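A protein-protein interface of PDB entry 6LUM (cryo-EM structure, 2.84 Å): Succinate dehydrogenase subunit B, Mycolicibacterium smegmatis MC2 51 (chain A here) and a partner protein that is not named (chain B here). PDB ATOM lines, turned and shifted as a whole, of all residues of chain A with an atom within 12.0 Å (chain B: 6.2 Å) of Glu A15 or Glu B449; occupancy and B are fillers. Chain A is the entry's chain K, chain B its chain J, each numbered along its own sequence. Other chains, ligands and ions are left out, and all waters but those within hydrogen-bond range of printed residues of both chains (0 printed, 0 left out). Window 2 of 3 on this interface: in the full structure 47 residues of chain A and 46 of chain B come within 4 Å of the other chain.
Printed residues of chain A that touch a printed residue of chain B: Glu A15, Leu A16, Pro A17 and Tyr A66.
Hydrophobic or aromatic side chains of chain A that line the printed part of chain B: Tyr A66.
Among the printed residues, no Asp or Glu carboxylate lies within 4 Å of a Lys or Arg side-chain nitrogen of the other chain.
The side-chain carboxylate of Glu A15 sits close to the side-chain carboxylate of Asp B453 (3.3 Å).
The backbone carbonyl oxygen (O) of Leu A16 is in hydrogen-bond range of the guanidinium group (NH2) of Arg B450, at 2.8 Å.
OE1 of Glu B449 sits at hydrogen-bond distance from ND2 of Asn B448.
The side-chain carboxylate (OD1) of Asp B453 is in salt-bridge range of the guanidinium group (NH1) of Arg B488 (3.98 Å).
The side-chain carboxylate (OE2) of Glu B449 lies within salt-bridge range of the guanidinium group (NE) of Arg B488, 3.1 Å away.
Among the printed residues, pairs that only touch across the chains: Glu A15 with Glu B449 (3.6 Å), Glu A15 with Asn B448 (3.7 Å), Tyr A66 with Arg B450 (3.8 Å) and Pro A17 with Arg B450 (3.99 Å).
Of chain B, only Asn B448, Glu B449 and Asp B453 come within 4 Å of Glu A15.
Of chain A, only Glu A15 comes within 4 Å of Glu B449.
Gly B447 touches none of the printed residues of chain A.
No residue of chain A comes within 4 Å of Val B451.
Asp B453 touches just one residue of chain A: Glu A15 (3.3 Å).
No residue of chain A comes within 4 Å of Arg B491.
No residue of chain A comes within 4 Å of Ile B492.
No residue of chain A comes within 4 Å of Thr B493.
Of the printed residues of chain B, Pro A17 touches Arg B450.
Printed residues of chain B within 4 Å of Leu A16: Arg B450.
Of the printed residues of chain A, Arg B450 touches Leu A16 (2.8 Å), Pro A17 (3.99 Å) and Tyr A66 (3.8 Å).
Of the printed residues of chain B, Tyr A66 touches Arg B450.
The nearest residue of chain A that does not touch Glu B449 is Pro A14 (5.0 Å).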
ATOM      1  N   PRO A  14      21.310  -8.274 -28.363  1.00  0.00           N
ATOM      2  CA  PRO A  14      22.367  -8.598 -27.403  1.00  0.00           C
ATOM      3  C   PRO A  14      23.524  -9.360 -28.028  1.00  0.00           C
ATOM      4  O   PRO A  14      23.894  -9.067 -29.163  1.00  0.00           O
ATOM      5  CB  PRO A  14      21.640  -9.454 -26.373  1.00  0.00           C
ATOM      6  CG  PRO A  14      20.267  -8.866 -26.344  1.00  0.00           C
ATOM      7  CD  PRO A  14      19.974  -8.372 -27.751  1.00  0.00           C
ATOM      8  N   GLU A  15      24.085 -10.322 -27.297  1.00  0.00           N
ATOM      9  CA  GLU A  15      25.349 -10.922 -27.705  1.00  0.00           C
ATOM     10  C   GLU A  15      25.272 -11.655 -29.038  1.00  0.00           C
ATOM     11  O   GLU A  15      25.784 -11.163 -30.048  1.00  0.00           O
ATOM     12  CB  GLU A  15      25.825 -11.894 -26.625  1.00  0.00           C
ATOM     13  CG  GLU A  15      26.210 -11.240 -25.313  1.00  0.00           C
ATOM     14  CD  GLU A  15      26.588 -12.255 -24.255  1.00  0.00           C
ATOM     15  OE1 GLU A  15      26.392 -13.464 -24.495  1.00  0.00           O
ATOM     16  OE2 GLU A  15      27.086 -11.848 -23.186  1.00  0.00           O
ATOM     17  N   LEU A  16      24.605 -12.807 -29.059  1.00  0.00           N
ATOM     18  CA  LEU A  16      24.501 -13.640 -30.251  1.00  0.00           C
ATOM     19  C   LEU A  16      23.603 -14.839 -29.971  1.00  0.00           C
ATOM     20  O   LEU A  16      23.615 -15.372 -28.855  1.00  0.00           O
ATOM     21  CB  LEU A  16      25.884 -14.101 -30.718  1.00  0.00           C
ATOM     22  CG  LEU A  16      26.566 -15.278 -30.019  1.00  0.00           C
ATOM     23  CD1 LEU A  16      27.814 -15.685 -30.783  1.00  0.00           C
ATOM     24  CD2 LEU A  16      26.915 -14.945 -28.581  1.00  0.00           C
ATOM     25  N   PRO A  17      22.812 -15.290 -30.938  1.00  0.00           N
ATOM     26  CA  PRO A  17      22.066 -16.536 -30.761  1.00  0.00           C
ATOM     27  C   PRO A  17      23.010 -17.722 -30.701  1.00  0.00           C
ATOM     28  O   PRO A  17      24.159 -17.634 -31.161  1.00  0.00           O
ATOM     29  CB  PRO A  17      21.159 -16.591 -32.001  1.00  0.00           C
ATOM     30  CG  PRO A  17      21.724 -15.606 -32.959  1.00  0.00           C
ATOM     31  CD  PRO A  17      22.390 -14.555 -32.141  1.00  0.00           C
ATOM     32  N   PRO A  18      22.566 -18.851 -30.136  1.00  0.00           N
ATOM     33  CA  PRO A  18      23.479 -19.980 -29.903  1.00  0.00           C
ATOM     34  C   PRO A  18      23.931 -20.675 -31.175  1.00  0.00           C
ATOM     35  O   PRO A  18      23.699 -20.194 -32.287  1.00  0.00           O
ATOM     36  CB  PRO A  18      22.650 -20.932 -29.031  1.00  0.00           C
ATOM     37  CG  PRO A  18      21.508 -20.137 -28.550  1.00  0.00           C
ATOM     38  CD  PRO A  18      21.231 -19.118 -29.590  1.00  0.00           C
ATOM     39  N   VAL A  19      24.585 -21.812 -30.998  1.00  0.00           N
ATOM     40  CA  VAL A  19      25.191 -22.581 -32.080  1.00  0.00           C
ATOM     41  C   VAL A  19      24.244 -23.719 -32.442  1.00  0.00           C
ATOM     42  O   VAL A  19      23.800 -24.447 -31.548  1.00  0.00           O
ATOM     43  CB  VAL A  19      26.568 -23.136 -31.669  1.00  0.00           C
ATOM     44  CG1 VAL A  19      27.174 -23.967 -32.786  1.00  0.00           C
ATOM     45  CG2 VAL A  19      27.489 -21.993 -31.260  1.00  0.00           C
ATOM     46  N   TYR A  62      12.663 -20.790 -28.709  1.00  0.00           N
ATOM     47  CA  TYR A  62      13.769 -20.156 -29.419  1.00  0.00           C
ATOM     48  C   TYR A  62      13.391 -18.756 -29.879  1.00  0.00           C
ATOM     49  O   TYR A  62      14.140 -17.798 -29.667  1.00  0.00           O
ATOM     50  CB  TYR A  62      14.183 -21.014 -30.610  1.00  0.00           C
ATOM     51  CG  TYR A  62      15.457 -20.588 -31.290  1.00  0.00           C
ATOM     52  CD1 TYR A  62      15.512 -19.436 -32.055  1.00  0.00           C
ATOM     53  CD2 TYR A  62      16.598 -21.356 -31.190  1.00  0.00           C
ATOM     54  CE1 TYR A  62      16.667 -19.056 -32.681  1.00  0.00           C
ATOM     55  CE2 TYR A  62      17.758 -20.982 -31.815  1.00  0.00           C
ATOM     56  CZ  TYR A  62      17.786 -19.833 -32.559  1.00  0.00           C
ATOM     57  OH  TYR A  62      18.948 -19.461 -33.184  1.00  0.00           O
ATOM     58  N   LYS A  64      11.041 -16.707 -28.770  1.00  0.00           N
ATOM     59  CA  LYS A  64      10.781 -15.767 -27.687  1.00  0.00           C
ATOM     60  C   LYS A  64      12.056 -15.397 -26.949  1.00  0.00           C
ATOM     61  O   LYS A  64      12.216 -14.253 -26.512  1.00  0.00           O
ATOM     62  CB  LYS A  64       9.766 -16.357 -26.721  1.00  0.00           C
ATOM     63  CG  LYS A  64       9.466 -15.468 -25.554  1.00  0.00           C
ATOM     64  CD  LYS A  64       8.354 -16.032 -24.718  1.00  0.00           C
ATOM     65  CE  LYS A  64       8.006 -15.083 -23.607  1.00  0.00           C
ATOM     66  NZ  LYS A  64       8.165 -13.690 -24.068  1.00  0.00           N
ATOM     67  N   TRP A  65      12.976 -16.340 -26.795  1.00  0.00           N
ATOM     68  CA  TRP A  65      14.195 -16.038 -26.065  1.00  0.00           C
ATOM     69  C   TRP A  65      15.140 -15.193 -26.901  1.00  0.00           C
ATOM     70  O   TRP A  65      15.571 -14.122 -26.466  1.00  0.00           O
ATOM     71  CB  TRP A  65      14.880 -17.328 -25.618  1.00  0.00           C
ATOM     72  CG  TRP A  65      14.099 -18.095 -24.616  1.00  0.00           C
ATOM     73  CD1 TRP A  65      13.044 -17.649 -23.888  1.00  0.00           C
ATOM     74  CD2 TRP A  65      14.304 -19.450 -24.231  1.00  0.00           C
ATOM     75  NE1 TRP A  65      12.577 -18.640 -23.074  1.00  0.00           N
ATOM     76  CE2 TRP A  65      13.336 -19.760 -23.267  1.00  0.00           C
ATOM     77  CE3 TRP A  65      15.212 -20.434 -24.610  1.00  0.00           C
ATOM     78  CZ2 TRP A  65      13.249 -21.006 -22.681  1.00  0.00           C
ATOM     79  CZ3 TRP A  65      15.126 -21.667 -24.027  1.00  0.00           C
ATOM     80  CH2 TRP A  65      14.155 -21.946 -23.072  1.00  0.00           C
ATOM     81  N   TYR A  66      15.458 -15.640 -28.114  1.00  0.00           N
ATOM     82  CA  TYR A  66      16.538 -14.998 -28.851  1.00  0.00           C
ATOM     83  C   TYR A  66      16.047 -13.914 -29.808  1.00  0.00           C
ATOM     84  O   TYR A  66      16.407 -12.743 -29.654  1.00  0.00           O
ATOM     85  CB  TYR A  66      17.347 -16.069 -29.577  1.00  0.00           C
ATOM     86  CG  TYR A  66      17.854 -17.110 -28.621  1.00  0.00           C
ATOM     87  CD1 TYR A  66      17.237 -18.335 -28.512  1.00  0.00           C
ATOM     88  CD2 TYR A  66      18.931 -16.853 -27.802  1.00  0.00           C
ATOM     89  CE1 TYR A  66      17.687 -19.284 -27.631  1.00  0.00           C
ATOM     90  CE2 TYR A  66      19.391 -17.794 -26.915  1.00  0.00           C
ATOM     91  CZ  TYR A  66      18.764 -19.008 -26.835  1.00  0.00           C
ATOM     92  OH  TYR A  66      19.217 -19.957 -25.952  1.00  0.00           O
ATOM     93  N   LEU A  67      15.217 -14.269 -30.786  1.00  0.00           N
ATOM     94  CA  LEU A  67      14.890 -13.307 -31.834  1.00  0.00           C
ATOM     95  C   LEU A  67      13.914 -12.246 -31.343  1.00  0.00           C
ATOM     96  O   LEU A  67      14.247 -11.060 -31.280  1.00  0.00           O
ATOM     97  CB  LEU A  67      14.312 -14.031 -33.049  1.00  0.00           C
ATOM     98  CG  LEU A  67      14.967 -15.347 -33.438  1.00  0.00           C
ATOM     99  CD1 LEU A  67      14.087 -16.085 -34.403  1.00  0.00           C
ATOM    100  CD2 LEU A  67      16.320 -15.103 -34.042  1.00  0.00           C
ATOM    101  N   ASP A  68      12.702 -12.658 -30.999  1.00  0.00           N
ATOM    102  CA  ASP A  68      11.664 -11.763 -30.507  1.00  0.00           C
ATOM    103  C   ASP A  68      11.685 -11.713 -28.989  1.00  0.00           C
ATOM    104  O   ASP A  68      12.739 -11.881 -28.373  1.00  0.00           O
ATOM    105  CB  ASP A  68      10.281 -12.155 -31.013  1.00  0.00           C
ATOM    106  CG  ASP A  68       9.419 -10.945 -31.291  1.00  0.00           C
ATOM    107  OD1 ASP A  68       9.593  -9.933 -30.589  1.00  0.00           O
ATOM    108  OD2 ASP A  68       8.581 -10.990 -32.212  1.00  0.00           O
ATOM    109  N   GLY A  69      10.538 -11.445 -28.381  1.00  0.00           N
ATOM    110  CA  GLY A  69      10.472 -11.226 -26.956  1.00  0.00           C
ATOM    111  C   GLY A  69       9.268 -10.402 -26.589  1.00  0.00           C
ATOM    112  O   GLY A  69       8.951 -10.231 -25.411  1.00  0.00           O
ATOM    113  N   GLY B 447      20.862  -3.449 -21.050  1.00  0.00           N
ATOM    114  CA  GLY B 447      22.141  -4.061 -20.763  1.00  0.00           C
ATOM    115  C   GLY B 447      22.496  -5.095 -21.810  1.00  0.00           C
ATOM    116  O   GLY B 447      21.678  -5.471 -22.650  1.00  0.00           O
ATOM    117  N   ASN B 448      23.741  -5.562 -21.731  1.00  0.00           N
ATOM    118  CA  ASN B 448      24.304  -6.480 -22.712  1.00  0.00           C
ATOM    119  C   ASN B 448      24.171  -7.944 -22.305  1.00  0.00           C
ATOM    120  O   ASN B 448      25.007  -8.769 -22.695  1.00  0.00           O
ATOM    121  CB  ASN B 448      25.770  -6.130 -22.956  1.00  0.00           C
ATOM    122  CG  ASN B 448      26.544  -5.967 -21.668  1.00  0.00           C
ATOM    123  OD1 ASN B 448      26.245  -5.086 -20.861  1.00  0.00           O
ATOM    124  ND2 ASN B 448      27.542  -6.818 -21.463  1.00  0.00           N
ATOM    125  N   GLU B 449      23.150  -8.288 -21.528  1.00  0.00           N
ATOM    126  CA  GLU B 449      22.931  -9.653 -21.078  1.00  0.00           C
ATOM    127  C   GLU B 449      21.498 -10.053 -21.377  1.00  0.00           C
ATOM    128  O   GLU B 449      20.596  -9.212 -21.357  1.00  0.00           O
ATOM    129  CB  GLU B 449      23.202  -9.797 -19.583  1.00  0.00           C
ATOM    130  CG  GLU B 449      24.580  -9.353 -19.151  1.00  0.00           C
ATOM    131  CD  GLU B 449      25.680 -10.151 -19.813  1.00  0.00           C
ATOM    132  OE1 GLU B 449      26.574  -9.541 -20.432  1.00  0.00           O
ATOM    133  OE2 GLU B 449      25.649 -11.393 -19.716  1.00  0.00           O
ATOM    134  N   ARG B 450      21.284 -11.334 -21.650  1.00  0.00           N
ATOM    135  CA  ARG B 450      19.949 -11.846 -21.904  1.00  0.00           C
ATOM    136  C   ARG B 450      19.585 -12.904 -20.873  1.00  0.00           C
ATOM    137  O   ARG B 450      20.406 -13.760 -20.510  1.00  0.00           O
ATOM    138  CB  ARG B 450      19.821 -12.408 -23.321  1.00  0.00           C
ATOM    139  CG  ARG B 450      20.871 -13.412 -23.706  1.00  0.00           C
ATOM    140  CD  ARG B 450      20.367 -14.300 -24.822  1.00  0.00           C
ATOM    141  NE  ARG B 450      19.917 -13.516 -25.961  1.00  0.00           N
ATOM    142  CZ  ARG B 450      20.558 -13.459 -27.119  1.00  0.00           C
ATOM    143  NH1 ARG B 450      20.083 -12.716 -28.104  1.00  0.00           N
ATOM    144  NH2 ARG B 450      21.673 -14.151 -27.290  1.00  0.00           N
ATOM    145  N   VAL B 451      18.337 -12.821 -20.408  1.00  0.00           N
ATOM    146  CA  VAL B 451      17.833 -13.735 -19.395  1.00  0.00           C
ATOM    147  C   VAL B 451      18.025 -15.174 -19.829  1.00  0.00           C
ATOM    148  O   VAL B 451      18.334 -16.045 -19.015  1.00  0.00           O
ATOM    149  CB  VAL B 451      16.355 -13.436 -19.106  1.00  0.00           C
ATOM    150  CG1 VAL B 451      15.840 -14.366 -18.063  1.00  0.00           C
ATOM    151  CG2 VAL B 451      16.192 -12.009 -18.672  1.00  0.00           C
ATOM    152  N   ASP B 453      20.409 -16.489 -21.630  1.00  0.00           N
ATOM    153  CA  ASP B 453      21.780 -16.955 -21.480  1.00  0.00           C
ATOM    154  C   ASP B 453      22.158 -17.078 -20.013  1.00  0.00           C
ATOM    155  O   ASP B 453      22.820 -18.048 -19.619  1.00  0.00           O
ATOM    156  CB  ASP B 453      22.737 -16.016 -22.209  1.00  0.00           C
ATOM    157  CG  ASP B 453      24.142 -16.586 -22.342  1.00  0.00           C
ATOM    158  OD1 ASP B 453      24.526 -17.483 -21.566  1.00  0.00           O
ATOM    159  OD2 ASP B 453      24.871 -16.129 -23.247  1.00  0.00           O
ATOM    160  N   ILE B 454      21.740 -16.121 -19.183  1.00  0.00           N
ATOM    161  CA  ILE B 454      22.028 -16.228 -17.754  1.00  0.00           C
ATOM    162  C   ILE B 454      21.396 -17.486 -17.181  1.00  0.00           C
ATOM    163  O   ILE B 454      22.040 -18.254 -16.460  1.00  0.00           O
ATOM    164  CB  ILE B 454      21.547 -14.977 -17.006  1.00  0.00           C
ATOM    165  CG1 ILE B 454      22.363 -13.769 -17.420  1.00  0.00           C
ATOM    166  CG2 ILE B 454      21.691 -15.174 -15.528  1.00  0.00           C
ATOM    167  CD1 ILE B 454      21.934 -12.541 -16.728  1.00  0.00           C
ATOM    168  N   ARG B 488      26.014 -10.564 -13.093  1.00  0.00           N
ATOM    169  CA  ARG B 488      25.569 -10.307 -14.460  1.00  0.00           C
ATOM    170  C   ARG B 488      24.079 -10.015 -14.529  1.00  0.00           C
ATOM    171  O   ARG B 488      23.637  -9.288 -15.418  1.00  0.00           O
ATOM    172  CB  ARG B 488      25.893 -11.492 -15.364  1.00  0.00           C
ATOM    173  CG  ARG B 488      27.302 -11.488 -15.900  1.00  0.00           C
ATOM    174  CD  ARG B 488      27.652 -12.827 -16.503  1.00  0.00           C
ATOM    175  NE  ARG B 488      26.610 -13.296 -17.406  1.00  0.00           N
ATOM    176  CZ  ARG B 488      26.718 -14.375 -18.167  1.00  0.00           C
ATOM    177  NH1 ARG B 488      25.724 -14.727 -18.964  1.00  0.00           N
ATOM    178  NH2 ARG B 488      27.821 -15.103 -18.130  1.00  0.00           N
ATOM    179  N   TYR B 489      23.294 -10.571 -13.610  1.00  0.00           N
ATOM    180  CA  TYR B 489      21.857 -10.333 -13.602  1.00  0.00           C
ATOM    181  C   TYR B 489      21.510  -8.883 -13.298  1.00  0.00           C
ATOM    182  O   TYR B 489      20.370  -8.471 -13.520  1.00  0.00           O
ATOM    183  CB  TYR B 489      21.196 -11.265 -12.587  1.00  0.00           C
ATOM    184  CG  TYR B 489      19.723 -11.041 -12.376  1.00  0.00           C
ATOM    185  CD1 TYR B 489      18.798 -11.511 -13.278  1.00  0.00           C
ATOM    186  CD2 TYR B 489      19.261 -10.363 -11.271  1.00  0.00           C
ATOM    187  CE1 TYR B 489      17.459 -11.309 -13.086  1.00  0.00           C
ATOM    188  CE2 TYR B 489      17.924 -10.158 -11.072  1.00  0.00           C
ATOM    189  CZ  TYR B 489      17.028 -10.634 -11.982  1.00  0.00           C
ATOM    190  OH  TYR B 489      15.687 -10.429 -11.787  1.00  0.00           O
ATOM    191  N   ARG B 491      22.462  -6.258 -14.871  1.00  0.00           N
ATOM    192  CA  ARG B 491      22.330  -5.497 -16.113  1.00  0.00           C
ATOM    193  C   ARG B 491      21.759  -6.420 -17.188  1.00  0.00           C
ATOM    194  O   ARG B 491      22.490  -6.982 -18.007  1.00  0.00           O
ATOM    195  CB  ARG B 491      23.671  -4.909 -16.520  1.00  0.00           C
ATOM    196  CG  ARG B 491      24.829  -5.877 -16.407  1.00  0.00           C
ATOM    197  CD  ARG B 491      26.104  -5.310 -16.995  1.00  0.00           C
ATOM    198  NE  ARG B 491      27.076  -6.355 -17.304  1.00  0.00           N
ATOM    199  CZ  ARG B 491      27.828  -6.970 -16.399  1.00  0.00           C
ATOM    200  NH1 ARG B 491      27.723  -6.650 -15.118  1.00  0.00           N
ATOM    201  NH2 ARG B 491      28.688  -7.906 -16.771  1.00  0.00           N
ATOM    202  N   ILE B 492      20.437  -6.556 -17.202  1.00  0.00           N
ATOM    203  CA  ILE B 492      19.737  -7.296 -18.239  1.00  0.00           C
ATOM    204  C   ILE B 492      18.667  -6.392 -18.829  1.00  0.00           C
ATOM    205  O   ILE B 492      18.327  -5.345 -18.281  1.00  0.00           O
ATOM    206  CB  ILE B 492      19.102  -8.604 -17.732  1.00  0.00           C
ATOM    207  CG1 ILE B 492      18.257  -8.345 -16.492  1.00  0.00           C
ATOM    208  CG2 ILE B 492      20.147  -9.636 -17.471  1.00  0.00           C
ATOM    209  CD1 ILE B 492      17.248  -9.411 -16.243  1.00  0.00           C
ATOM    210  N   THR B 493      18.123  -6.827 -19.952  1.00  0.00           N
ATOM    211  CA  THR B 493      17.135  -6.064 -20.684  1.00  0.00           C
ATOM    212  C   THR B 493      15.881  -6.895 -20.898  1.00  0.00           C
ATOM    213  O   THR B 493      15.928  -8.127 -20.939  1.00  0.00           O
ATOM    214  CB  THR B 493      17.690  -5.610 -22.032  1.00  0.00           C
ATOM    215  OG1 THR B 493      16.703  -4.833 -22.720  1.00  0.00           O
ATOM    216  CG2 THR B 493      18.084  -6.808 -22.876  1.00  0.00           C
